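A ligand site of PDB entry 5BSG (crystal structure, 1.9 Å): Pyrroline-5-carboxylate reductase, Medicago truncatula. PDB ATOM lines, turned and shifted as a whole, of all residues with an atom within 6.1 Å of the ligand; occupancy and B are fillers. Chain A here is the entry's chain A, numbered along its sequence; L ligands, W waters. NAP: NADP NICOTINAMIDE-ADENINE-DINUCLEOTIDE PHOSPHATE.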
ATOM      1  N   ILE A  19      25.910 -11.876 -10.215  1.00  0.00           N
ATOM      2  CA  ILE A  19      25.843 -13.278 -10.531  1.00  0.00           C
ATOM      3  C   ILE A  19      26.051 -14.054  -9.231  1.00  0.00           C
ATOM      4  O   ILE A  19      27.163 -14.135  -8.696  1.00  0.00           O
ATOM      5  CB  ILE A  19      26.893 -13.695 -11.558  1.00  0.00           C
ATOM      6  CG1 ILE A  19      26.797 -12.837 -12.808  1.00  0.00           C
ATOM      7  CG2 ILE A  19      26.772 -15.190 -11.899  1.00  0.00           C
ATOM      8  CD1 ILE A  19      25.502 -12.952 -13.565  1.00  0.00           C
ATOM      9  N   GLY A  20      24.979 -14.629  -8.721  1.00  0.00           N
ATOM     10  CA  GLY A  20      24.954 -15.282  -7.396  1.00  0.00           C
ATOM     11  C   GLY A  20      24.197 -14.398  -6.445  1.00  0.00           C
ATOM     12  O   GLY A  20      24.737 -13.454  -5.860  1.00  0.00           O
ATOM     13  N   ALA A  21      22.901 -14.641  -6.373  1.00  0.00           N
ATOM     14  CA  ALA A  21      21.993 -13.750  -5.667  1.00  0.00           C
ATOM     15  C   ALA A  21      21.920 -14.067  -4.156  1.00  0.00           C
ATOM     16  O   ALA A  21      20.826 -14.247  -3.600  1.00  0.00           O
ATOM     17  CB  ALA A  21      20.596 -13.834  -6.313  1.00  0.00           C
ATOM     18  N   GLY A  22      23.083 -14.144  -3.498  1.00  0.00           N
ATOM     19  CA  GLY A  22      23.148 -14.568  -2.096  1.00  0.00           C
ATOM     20  C   GLY A  22      23.144 -13.445  -1.102  1.00  0.00           C
ATOM     21  O   GLY A  22      22.800 -12.297  -1.414  1.00  0.00           O
ATOM     22  N   LYS A  23      23.628 -13.717   0.079  1.00  0.00           N
ATOM     23  CA  LYS A  23      23.703 -12.758   1.130  1.00  0.00           C
ATOM     24  C   LYS A  23      24.653 -11.593   0.839  1.00  0.00           C
ATOM     25  O   LYS A  23      24.305 -10.508   1.093  1.00  0.00           O
ATOM     26  CB  LYS A  23      24.096 -13.429   2.436  1.00  0.00           C
ATOM     27  CG  LYS A  23      23.232 -14.626   2.808  1.00  0.00           C
ATOM     28  CD  LYS A  23      23.952 -15.447   3.877  1.00  0.00           C
ATOM     29  CE  LYS A  23      24.510 -16.784   3.422  1.00  0.00           C
ATOM     30  NZ  LYS A  23      25.963 -16.669   3.540  1.00  0.00           N
ATOM     31  N   MET A  24      25.844 -11.886   0.355  1.00  0.00           N
ATOM     32  CA  MET A  24      26.810 -10.801   0.089  1.00  0.00           C
ATOM     33  C   MET A  24      26.304  -9.858  -1.056  1.00  0.00           C
ATOM     34  O   MET A  24      26.361  -8.646  -0.930  1.00  0.00           O
ATOM     35  CB  MET A  24      28.221 -11.348  -0.212  1.00  0.00           C
ATOM     36  CG  MET A  24      29.254 -10.257  -0.451  1.00  0.00           C
ATOM     37  SD  MET A  24      29.477  -8.934   0.825  1.00  0.00           S
ATOM     38  CE  MET A  24      30.069  -9.999   2.128  1.00  0.00           C
ATOM     39  N   ALA A  25      25.764 -10.452  -2.104  1.00  0.00           N
ATOM     40  CA  ALA A  25      25.127  -9.655  -3.155  1.00  0.00           C
ATOM     41  C   ALA A  25      24.020  -8.753  -2.604  1.00  0.00           C
ATOM     42  O   ALA A  25      23.955  -7.573  -2.911  1.00  0.00           O
ATOM     43  CB  ALA A  25      24.555 -10.567  -4.262  1.00  0.00           C
ATOM     44  N   ALA A  46      19.898 -12.770 -11.010  1.00  0.00           N
ATOM     45  CA  ALA A  46      19.147 -13.923 -11.465  1.00  0.00           C
ATOM     46  C   ALA A  46      19.288 -14.988 -10.418  1.00  0.00           C
ATOM     47  O   ALA A  46      20.348 -15.104  -9.823  1.00  0.00           O
ATOM     48  CB  ALA A  46      19.631 -14.454 -12.805  1.00  0.00           C
ATOM     49  N   ILE A  47      18.207 -15.735 -10.160  1.00  0.00           N
ATOM     50  CA  ILE A  47      18.251 -16.777  -9.151  1.00  0.00           C
ATOM     51  C   ILE A  47      18.831 -18.057  -9.700  1.00  0.00           C
ATOM     52  O   ILE A  47      18.927 -18.238 -10.869  1.00  0.00           O
ATOM     53  CB  ILE A  47      16.925 -17.014  -8.401  1.00  0.00           C
ATOM     54  CG1 ILE A  47      15.832 -17.609  -9.316  1.00  0.00           C
ATOM     55  CG2 ILE A  47      16.501 -15.693  -7.744  1.00  0.00           C
ATOM     56  CD1 ILE A  47      15.034 -18.765  -8.712  1.00  0.00           C
ATOM     57  N   HIS A  48      19.179 -18.963  -8.822  1.00  0.00           N
ATOM     58  CA  HIS A  48      19.635 -20.283  -9.235  1.00  0.00           C
ATOM     59  C   HIS A  48      18.518 -21.322  -8.950  1.00  0.00           C
ATOM     60  O   HIS A  48      17.617 -21.460  -9.775  1.00  0.00           O
ATOM     61  CB  HIS A  48      20.982 -20.588  -8.550  1.00  0.00           C
ATOM     62  CG  HIS A  48      21.625 -21.870  -8.978  1.00  0.00           C
ATOM     63  ND1 HIS A  48      22.031 -22.833  -8.077  1.00  0.00           N
ATOM     64  CD2 HIS A  48      21.955 -22.332 -10.198  1.00  0.00           C
ATOM     65  CE1 HIS A  48      22.568 -23.838  -8.731  1.00  0.00           C
ATOM     66  NE2 HIS A  48      22.535 -23.569 -10.023  1.00  0.00           N
ATOM     67  N   SER A  49      18.521 -21.948  -7.792  1.00  0.00           N
ATOM     68  CA  SER A  49      17.506 -22.972  -7.426  1.00  0.00           C
ATOM     69  C   SER A  49      16.516 -22.493  -6.330  1.00  0.00           C
ATOM     70  O   SER A  49      15.332 -22.742  -6.437  1.00  0.00           O
ATOM     71  CB  SER A  49      18.179 -24.258  -6.962  1.00  0.00           C
ATOM     72  OG  SER A  49      18.751 -24.085  -5.690  1.00  0.00           O
ATOM     73  N   ASN A  50      17.024 -21.723  -5.372  1.00  0.00           N
ATOM     74  CA  ASN A  50      16.239 -21.181  -4.297  1.00  0.00           C
ATOM     75  C   ASN A  50      15.354 -19.974  -4.670  1.00  0.00           C
ATOM     76  O   ASN A  50      15.835 -18.866  -4.838  1.00  0.00           O
ATOM     77  CB  ASN A  50      17.212 -20.791  -3.221  1.00  0.00           C
ATOM     78  CG  ASN A  50      16.520 -20.295  -1.987  1.00  0.00           C
ATOM     79  OD1 ASN A  50      15.271 -20.210  -1.907  1.00  0.00           O
ATOM     80  ND2 ASN A  50      17.311 -19.870  -1.050  1.00  0.00           N
ATOM     81  N   PRO A  51      14.024 -20.169  -4.757  1.00  0.00           N
ATOM     82  CA  PRO A  51      13.135 -19.051  -5.126  1.00  0.00           C
ATOM     83  C   PRO A  51      12.935 -18.002  -4.057  1.00  0.00           C
ATOM     84  O   PRO A  51      12.358 -16.940  -4.312  1.00  0.00           O
ATOM     85  CB  PRO A  51      11.804 -19.763  -5.391  1.00  0.00           C
ATOM     86  CG  PRO A  51      11.804 -20.912  -4.433  1.00  0.00           C
ATOM     87  CD  PRO A  51      13.253 -21.365  -4.341  1.00  0.00           C
ATOM     88  N   ARG A  53      15.290 -16.352  -2.752  1.00  0.00           N
ATOM     89  CA  ARG A  53      16.238 -15.281  -3.120  1.00  0.00           C
ATOM     90  C   ARG A  53      15.560 -14.293  -4.045  1.00  0.00           C
ATOM     91  O   ARG A  53      15.867 -13.123  -4.034  1.00  0.00           O
ATOM     92  CB  ARG A  53      17.507 -15.828  -3.742  1.00  0.00           C
ATOM     93  CG  ARG A  53      18.298 -16.800  -2.882  1.00  0.00           C
ATOM     94  CD  ARG A  53      18.485 -16.251  -1.480  1.00  0.00           C
ATOM     95  NE  ARG A  53      19.153 -14.978  -1.477  1.00  0.00           N
ATOM     96  CZ  ARG A  53      19.057 -14.030  -0.525  1.00  0.00           C
ATOM     97  NH1 ARG A  53      18.293 -14.206   0.534  1.00  0.00           N
ATOM     98  NH2 ARG A  53      19.815 -12.948  -0.582  1.00  0.00           N
ATOM     99  N   ASN A  68      21.627 -15.959 -15.891  1.00  0.00           N
ATOM    100  CA  ASN A  68      22.897 -15.251 -15.698  1.00  0.00           C
ATOM    101  C   ASN A  68      23.270 -14.475 -16.960  1.00  0.00           C
ATOM    102  O   ASN A  68      23.781 -13.353 -16.889  1.00  0.00           O
ATOM    103  CB  ASN A  68      24.031 -16.190 -15.362  1.00  0.00           C
ATOM    104  CG  ASN A  68      23.928 -16.772 -13.980  1.00  0.00           C
ATOM    105  OD1 ASN A  68      23.089 -16.402 -13.149  1.00  0.00           O
ATOM    106  ND2 ASN A  68      24.730 -17.747 -13.751  1.00  0.00           N
ATOM    107  N   PHE A  80      30.662 -11.082  -9.484  1.00  0.00           N
ATOM    108  CA  PHE A  80      30.525 -12.499  -9.237  1.00  0.00           C
ATOM    109  C   PHE A  80      30.491 -12.777  -7.747  1.00  0.00           C
ATOM    110  O   PHE A  80      31.524 -12.560  -7.037  1.00  0.00           O
ATOM    111  CB  PHE A  80      31.678 -13.253  -9.897  1.00  0.00           C
ATOM    112  CG  PHE A  80      31.593 -13.219 -11.395  1.00  0.00           C
ATOM    113  CD1 PHE A  80      30.709 -14.058 -12.065  1.00  0.00           C
ATOM    114  CD2 PHE A  80      32.359 -12.325 -12.141  1.00  0.00           C
ATOM    115  CE1 PHE A  80      30.627 -13.980 -13.452  1.00  0.00           C
ATOM    116  CE2 PHE A  80      32.301 -12.270 -13.545  1.00  0.00           C
ATOM    117  CZ  PHE A  80      31.429 -13.084 -14.189  1.00  0.00           C
ATOM    118  N   SER A  81      29.354 -13.222  -7.266  1.00  0.00           N
ATOM    119  CA  SER A  81      29.139 -13.441  -5.837  1.00  0.00           C
ATOM    120  C   SER A  81      28.599 -14.849  -5.559  1.00  0.00           C
ATOM    121  O   SER A  81      27.722 -15.057  -4.678  1.00  0.00           O
ATOM    122  CB  SER A  81      28.130 -12.377  -5.262  1.00  0.00           C
ATOM    123  OG  SER A  81      27.055 -12.135  -6.186  1.00  0.00           O
ATOM    124  N   VAL A  82      29.099 -15.810  -6.316  1.00  0.00           N
ATOM    125  CA  VAL A  82      28.837 -17.211  -6.016  1.00  0.00           C
ATOM    126  C   VAL A  82      29.908 -17.770  -5.111  1.00  0.00           C
ATOM    127  O   VAL A  82      30.952 -17.153  -4.950  1.00  0.00           O
ATOM    128  CB  VAL A  82      28.724 -18.099  -7.316  1.00  0.00           C
ATOM    129  CG1 VAL A  82      27.559 -17.606  -8.205  1.00  0.00           C
ATOM    130  CG2 VAL A  82      30.012 -18.112  -8.097  1.00  0.00           C
ATOM    131  N   LYS A  83      29.668 -18.930  -4.518  1.00  0.00           N
ATOM    132  CA  LYS A  83      30.691 -19.576  -3.718  1.00  0.00           C
ATOM    133  C   LYS A  83      31.916 -19.892  -4.556  1.00  0.00           C
ATOM    134  O   LYS A  83      31.818 -20.187  -5.710  1.00  0.00           O
ATOM    135  CB  LYS A  83      30.198 -20.883  -3.150  1.00  0.00           C
ATOM    136  CG  LYS A  83      29.094 -20.765  -2.152  1.00  0.00           C
ATOM    137  CD  LYS A  83      29.465 -19.772  -1.098  1.00  0.00           C
ATOM    138  CE  LYS A  83      29.257 -20.331   0.276  1.00  0.00           C
ATOM    139  NZ  LYS A  83      27.890 -20.196   0.772  1.00  0.00           N
ATOM    140  N   PRO A  84      33.061 -19.851  -3.944  1.00  0.00           N
ATOM    141  CA  PRO A  84      34.291 -19.903  -4.715  1.00  0.00           C
ATOM    142  C   PRO A  84      34.434 -21.139  -5.579  1.00  0.00           C
ATOM    143  O   PRO A  84      34.966 -21.101  -6.724  1.00  0.00           O
ATOM    144  CB  PRO A  84      35.386 -19.905  -3.687  1.00  0.00           C
ATOM    145  CG  PRO A  84      34.746 -19.517  -2.446  1.00  0.00           C
ATOM    146  CD  PRO A  84      33.274 -19.695  -2.515  1.00  0.00           C
ATOM    147  N   LEU A  86      32.322 -22.737  -7.080  1.00  0.00           N
ATOM    148  CA  LEU A  86      31.438 -22.731  -8.244  1.00  0.00           C
ATOM    149  C   LEU A  86      31.783 -21.679  -9.285  1.00  0.00           C
ATOM    150  O   LEU A  86      31.218 -21.644 -10.406  1.00  0.00           O
ATOM    151  CB  LEU A  86      29.994 -22.469  -7.797  1.00  0.00           C
ATOM    152  CG  LEU A  86      29.409 -23.444  -6.797  1.00  0.00           C
ATOM    153  CD1 LEU A  86      27.946 -23.124  -6.467  1.00  0.00           C
ATOM    154  CD2 LEU A  86      29.538 -24.886  -7.284  1.00  0.00           C
ATOM    155  N   VAL A  90      30.934 -21.046 -13.687  1.00  0.00           N
ATOM    156  CA  VAL A  90      30.031 -19.958 -13.928  1.00  0.00           C
ATOM    157  C   VAL A  90      30.665 -18.973 -14.948  1.00  0.00           C
ATOM    158  O   VAL A  90      29.964 -18.520 -15.883  1.00  0.00           O
ATOM    159  CB  VAL A  90      29.689 -19.239 -12.603  1.00  0.00           C
ATOM    160  CG1 VAL A  90      29.169 -17.831 -12.848  1.00  0.00           C
ATOM    161  CG2 VAL A  90      28.711 -20.066 -11.831  1.00  0.00           C
ATOM    162  N   VAL A 107      33.985 -11.160  -5.654  1.00  0.00           N
ATOM    163  CA  VAL A 107      34.103 -11.094  -4.192  1.00  0.00           C
ATOM    164  C   VAL A 107      34.380 -12.499  -3.607  1.00  0.00           C
ATOM    165  O   VAL A 107      34.425 -12.665  -2.377  1.00  0.00           O
ATOM    166  CB  VAL A 107      32.876 -10.521  -3.491  1.00  0.00           C
ATOM    167  CG1 VAL A 107      32.669  -9.056  -3.929  1.00  0.00           C
ATOM    168  CG2 VAL A 107      31.610 -11.344  -3.789  1.00  0.00           C
ATOM    169  N   ALA A 108      34.685 -13.469  -4.466  1.00  0.00           N
ATOM    170  CA  ALA A 108      34.919 -14.851  -3.993  1.00  0.00           C
ATOM    171  C   ALA A 108      36.157 -14.993  -3.112  1.00  0.00           C
ATOM    172  O   ALA A 108      37.267 -14.547  -3.478  1.00  0.00           O
ATOM    173  CB  ALA A 108      35.011 -15.782  -5.175  1.00  0.00           C
ATOM    174  N   ALA A 109      35.984 -15.571  -1.937  1.00  0.00           N
ATOM    175  CA  ALA A 109      37.119 -15.753  -1.025  1.00  0.00           C
ATOM    176  C   ALA A 109      38.109 -16.732  -1.652  1.00  0.00           C
ATOM    177  O   ALA A 109      37.706 -17.737  -2.250  1.00  0.00           O
ATOM    178  CB  ALA A 109      36.637 -16.279   0.356  1.00  0.00           C
ATOM    179  N   GLY A 110      39.387 -16.393  -1.578  1.00  0.00           N
ATOM    180  CA  GLY A 110      40.452 -17.282  -1.944  1.00  0.00           C
ATOM    181  C   GLY A 110      40.716 -17.445  -3.466  1.00  0.00           C
ATOM    182  O   GLY A 110      41.534 -18.237  -3.809  1.00  0.00           O
ATOM    183  N   VAL A 128      37.694  -8.104  -4.970  1.00  0.00           N
ATOM    184  CA  VAL A 128      37.400  -7.533  -3.669  1.00  0.00           C
ATOM    185  C   VAL A 128      37.240  -8.630  -2.615  1.00  0.00           C
ATOM    186  O   VAL A 128      36.701  -9.680  -2.872  1.00  0.00           O
ATOM    187  CB  VAL A 128      36.149  -6.671  -3.680  1.00  0.00           C
ATOM    188  CG1 VAL A 128      35.943  -5.978  -2.375  1.00  0.00           C
ATOM    189  CG2 VAL A 128      36.254  -5.622  -4.756  1.00  0.00           C
ATOM    190  N   MET A 129      37.830  -8.397  -1.451  1.00  0.00           N
ATOM    191  CA  MET A 129      37.595  -9.263  -0.266  1.00  0.00           C
ATOM    192  C   MET A 129      36.951  -8.417   0.783  1.00  0.00           C
ATOM    193  O   MET A 129      37.602  -7.650   1.483  1.00  0.00           O
ATOM    194  CB  MET A 129      38.905  -9.882   0.238  1.00  0.00           C
ATOM    195  CG  MET A 129      38.785 -10.749   1.491  1.00  0.00           C
ATOM    196  SD  MET A 129      37.617 -12.078   1.156  1.00  0.00           S
ATOM    197  CE  MET A 129      37.480 -12.793   2.852  1.00  0.00           C
ATOM    198  N   PRO A 130      35.642  -8.459   0.854  1.00  0.00           N
ATOM    199  CA  PRO A 130      34.910  -7.867   1.939  1.00  0.00           C
ATOM    200  C   PRO A 130      34.880  -8.749   3.190  1.00  0.00           C
ATOM    201  O   PRO A 130      35.668  -9.700   3.287  1.00  0.00           O
ATOM    202  CB  PRO A 130      33.524  -7.725   1.358  1.00  0.00           C
ATOM    203  CG  PRO A 130      33.405  -8.944   0.489  1.00  0.00           C
ATOM    204  CD  PRO A 130      34.793  -9.322   0.021  1.00  0.00           C
ATOM    205  N   ASN A 131      34.101  -8.385   4.199  1.00  0.00           N
ATOM    206  CA  ASN A 131      33.924  -9.234   5.356  1.00  0.00           C
ATOM    207  C   ASN A 131      32.493  -9.143   5.847  1.00  0.00           C
ATOM    208  O   ASN A 131      31.641  -8.472   5.214  1.00  0.00           O
ATOM    209  CB  ASN A 131      34.970  -8.974   6.431  1.00  0.00           C
ATOM    210  CG  ASN A 131      34.723  -7.707   7.216  1.00  0.00           C
ATOM    211  OD1 ASN A 131      33.743  -6.986   7.052  1.00  0.00           O
ATOM    212  ND2 ASN A 131      35.635  -7.438   8.138  1.00  0.00           N
ATOM    213  N   THR A 132      32.229  -9.852   6.900  1.00  0.00           N
ATOM    214  CA  THR A 132      30.827 -10.127   7.341  1.00  0.00           C
ATOM    215  C   THR A 132      30.081  -8.814   7.690  1.00  0.00           C
ATOM    216  O   THR A 132      28.848  -8.787   7.697  1.00  0.00           O
ATOM    217  CB  THR A 132      30.816 -11.089   8.514  1.00  0.00           C
ATOM    218  OG1 THR A 132      29.480 -11.503   8.858  1.00  0.00           O
ATOM    219  CG2 THR A 132      31.414 -10.440   9.797  1.00  0.00           C
ATOM    220  N   ALA A 133      30.832  -7.777   8.063  1.00  0.00           N
ATOM    221  CA  ALA A 133      30.208  -6.598   8.606  1.00  0.00           C
ATOM    222  C   ALA A 133      29.626  -5.711   7.498  1.00  0.00           C
ATOM    223  O   ALA A 133      29.013  -4.666   7.757  1.00  0.00           O
ATOM    224  CB  ALA A 133      31.149  -5.813   9.474  1.00  0.00           C
ATOM    225  N   ALA A 134      29.721  -6.182   6.271  1.00  0.00           N
ATOM    226  CA  ALA A 134      28.956  -5.607   5.166  1.00  0.00           C
ATOM    227  C   ALA A 134      27.461  -5.419   5.504  1.00  0.00           C
ATOM    228  O   ALA A 134      26.851  -4.460   5.109  1.00  0.00           O
ATOM    229  CB  ALA A 134      29.090  -6.464   3.935  1.00  0.00           C
HETATM  230  PA  NAP L   1      25.417 -17.436  -0.558  1.00  0.00           P
HETATM  231  O1A NAP L   1      24.604 -16.674   0.325  1.00  0.00           O
HETATM  232  O2A NAP L   1      25.339 -18.853  -0.489  1.00  0.00           O
HETATM  233  O5B NAP L   1      25.100 -17.013  -2.050  1.00  0.00           O
HETATM  234  C5B NAP L   1      25.557 -17.738  -3.176  1.00  0.00           C
HETATM  235  C4B NAP L   1      24.461 -17.789  -4.229  1.00  0.00           C
HETATM  236  O4B NAP L   1      24.889 -18.316  -5.449  1.00  0.00           O
HETATM  237  C3B NAP L   1      23.320 -18.664  -3.769  1.00  0.00           C
HETATM  238  O3B NAP L   1      22.221 -17.819  -3.757  1.00  0.00           O
HETATM  239  C2B NAP L   1      23.207 -19.764  -4.813  1.00  0.00           C
HETATM  240  O2B NAP L   1      21.854 -20.151  -5.016  1.00  0.00           O
HETATM  241  C1B NAP L   1      23.842 -19.047  -5.990  1.00  0.00           C
HETATM  242  N9A NAP L   1      24.327 -19.878  -7.113  1.00  0.00           N
HETATM  243  C8A NAP L   1      24.813 -21.117  -7.076  1.00  0.00           C
HETATM  244  N7A NAP L   1      25.153 -21.527  -8.302  1.00  0.00           N
HETATM  245  C5A NAP L   1      24.900 -20.541  -9.128  1.00  0.00           C
HETATM  246  C6A NAP L   1      25.028 -20.307 -10.577  1.00  0.00           C
HETATM  247  N6A NAP L   1      25.525 -21.279 -11.321  1.00  0.00           N
HETATM  248  N1A NAP L   1      24.652 -19.124 -11.044  1.00  0.00           N
HETATM  249  C2A NAP L   1      24.179 -18.182 -10.244  1.00  0.00           C
HETATM  250  N3A NAP L   1      24.031 -18.306  -8.960  1.00  0.00           N
HETATM  251  C4A NAP L   1      24.355 -19.454  -8.353  1.00  0.00           C
HETATM  252  O3  NAP L   1      26.933 -16.991  -0.435  1.00  0.00           O
HETATM  253  PN  NAP L   1      27.427 -15.636   0.168  1.00  0.00           P
HETATM  254  O1N NAP L   1      27.662 -15.741   1.569  1.00  0.00           O
HETATM  255  O2N NAP L   1      26.596 -14.575  -0.273  1.00  0.00           O
HETATM  256  O5D NAP L   1      28.874 -15.664  -0.444  1.00  0.00           O
HETATM  257  C5D NAP L   1      29.173 -15.264  -1.755  1.00  0.00           C
HETATM  258  C4D NAP L   1      30.648 -14.953  -1.960  1.00  0.00           C
HETATM  259  O4D NAP L   1      31.041 -13.874  -1.170  1.00  0.00           O
HETATM  260  C3D NAP L   1      31.497 -16.159  -1.632  1.00  0.00           C
HETATM  261  O3D NAP L   1      32.462 -16.478  -2.611  1.00  0.00           O
HETATM  262  C2D NAP L   1      32.177 -15.739  -0.335  1.00  0.00           C
HETATM  263  O2D NAP L   1      33.453 -16.313  -0.262  1.00  0.00           O
HETATM  264  C1D NAP L   1      32.217 -14.236  -0.468  1.00  0.00           C
HETATM  265  N1N NAP L   1      32.322 -13.535   0.795  1.00  0.00           N
HETATM  266  C2N NAP L   1      31.295 -13.556   1.643  1.00  0.00           C
HETATM  267  C3N NAP L   1      31.392 -12.890   2.850  1.00  0.00           C
HETATM  268  C7N NAP L   1      30.174 -12.947   3.722  1.00  0.00           C
HETATM  269  O7N NAP L   1      30.139 -12.348   4.747  1.00  0.00           O
HETATM  270  N7N NAP L   1      29.148 -13.660   3.320  1.00  0.00           N
HETATM  271  C4N NAP L   1      32.572 -12.197   3.194  1.00  0.00           C
HETATM  272  C5N NAP L   1      33.648 -12.186   2.307  1.00  0.00           C
HETATM  273  C6N NAP L   1      33.442 -12.898   1.116  1.00  0.00           C
HETATM  274  P2B NAP L   1      21.250 -21.553  -4.683  1.00  0.00           P
HETATM  275  O1X NAP L   1      19.937 -21.417  -5.254  1.00  0.00           O
HETATM  276  O2X NAP L   1      22.079 -22.525  -5.407  1.00  0.00           O
HETATM  277  O3X NAP L   1      21.399 -21.614  -3.259  1.00  0.00           O
HETATM  278  O   HOH W   1      32.299 -14.029   6.907  1.00  0.00           O
HETATM  279  O   HOH W   2      22.860 -15.010 -10.750  1.00  0.00           O
HETATM  280  O   HOH W   3      21.706 -17.081   0.119  1.00  0.00           O
HETATM  281  O   HOH W   4      26.838 -23.404  -9.653  1.00  0.00           O
HETATM  282  O   HOH W   5      25.942 -13.397  -2.676  1.00  0.00           O
HETATM  283  O   HOH W   6      26.864 -12.164   4.655  1.00  0.00           O
HETATM  284  O   HOH W   7      21.778 -16.813  -8.055  1.00  0.00           O
HETATM  285  O   HOH W   8      30.055 -17.246   2.698  1.00  0.00           O
HETATM  286  O   HOH W   9      29.305 -13.519   7.033  1.00  0.00           O
HETATM  287  O   HOH W  10      20.565 -17.379  -5.658  1.00  0.00           O
HETATM  288  O   HOH W  11      27.036 -20.123  -4.911  1.00  0.00           O
HETATM  289  O   HOH W  12      26.295 -21.288 -14.193  1.00  0.00           O
HETATM  290  O   HOH W  13      20.277 -19.566  -1.868  1.00  0.00           O
HETATM  291  O   HOH W  14      21.590 -18.535 -11.885  1.00  0.00           O
HETATM  292  O   HOH W  15      18.833 -19.172  -5.960  1.00  0.00           O
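N of Ser 49 is in hydrogen-bond range of O1X of the ligand (3.0 Å).
ND2 of Asn 68 is in hydrogen-bond range of N1A of the ligand (3.0 Å).
An oxygen (O2N) of the ligand lies within hydrogen-bond range of the backbone NH (N) of Met 24 (2.9 Å).
O3D of the ligand sits at hydrogen-bond distance from O of Val 82 (2.9 Å).
The side-chain amino group (NZ) of Lys 23 is in salt-bridge range of an oxygen (O1N) of the ligand, 2.8 Å away.
The backbone NH (N) of Asn 50 sits at hydrogen-bond distance from an oxygen (O1X) of the ligand (2.9 Å).
N of Lys 23 is in hydrogen-bond range of O2N of the ligand.
The side-chain amino group of Lys 83 is in salt-bridge range of an oxygen (O2A) of the ligand (3.1 Å).
O2D of the ligand lies within hydrogen-bond range of N of Ala 109, 3.1 Å away.
O2X of the ligand lies within hydrogen-bond range of ND1 of His 48 (2.7 Å).
O1X of the ligand is in hydrogen-bond range of OG of Ser 49 (3.0 Å).
The backbone NH of Val 82 sits at hydrogen-bond distance from the backbone carbonyl oxygen of Ile 19 (3.5 Å).
The backbone carbonyl oxygen (O) of Ile 19 sits at hydrogen-bond distance from the backbone NH (N) of Ser 81, 2.8 Å away.
O of Phe 80 is in hydrogen-bond range of N of Val 107 (3.2 Å).
NH2 of Arg 53 is in hydrogen-bond range of O of Gly 22 (3.2 Å).
The backbone carbonyl oxygen (O) of Ala 21 sits at hydrogen-bond distance from the guanidinium group (NE) of Arg 53 (2.8 Å).
The side-chain hydroxyl (OG) of Ser 81 is in hydrogen-bond range of the backbone carbonyl oxygen (O) of Gly 20 (2.7 Å).
The side-chain amide oxygen (OD1) of Asn 131 lies close to the backbone NH (N) of Ala 133, at 3.2 Å.
Gly 20 touches the ligand.
Ala 21 touches the ligand.
CA of Gly 22 touches O5B of the ligand (3.1 Å).
Ser 81 touches the ligand.
CD of Pro 84 touches O3D of the ligand (3.3 Å).
CD1 of Leu 86 touches N7A of the ligand (3.7 Å).
Val 90 touches the ligand (CG2 to N6A, 3.4 Å).
Val 107 touches the ligand (O to C1D, 3.3 Å).
CA of Ala 108 touches O3D of the ligand, 3.3 Å away.
Met 129 touches the ligand (CE to C5N, 3.9 Å).
O of Pro 130 touches C5N of the ligand (3.3 Å).
Asn 131 touches the ligand.
Thr 132 touches the ligand (CA to O7N, 3.5 Å).
Hydrophobic or aromatic side chains that line the ligand: Met 24, His 48, Val 82, Pro 84, Leu 86, Val 90, Val 107, Ala 108, Ala 109, Met 129 and Pro 130.
Along chain A the residues within 4 Å of the ligand span positions 20 to 132.
Water W9 lies within hydrogen-bond range of an oxygen (O7N) of the ligand (2.7 Å) and the side-chain hydroxyl (OG1) of Thr 132 (2.7 Å).
Water W13 bridges an oxygen (O3X) of the ligand (2.7 Å) and the side-chain amide nitrogen (ND2) of Asn 50 (3.1 Å).
Water W7 lies within hydrogen-bond range of the backbone carbonyl oxygen of Ala 46 (2.8 Å), a nitrogen (N3A) of the ligand (2.9 Å), the backbone NH of Ala 21 (3.0 Å) and the backbone NH of His 48 (3.5 Å).
Water W11 bridges an oxygen (O4B) of the ligand and the backbone NH (N) of Lys 83.
Water W2 lies within hydrogen-bond range of the backbone carbonyl oxygen (O) of Ala 46, the side-chain amide oxygen (OD1) of Asn 68 and the backbone NH (N) of Gly 20.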
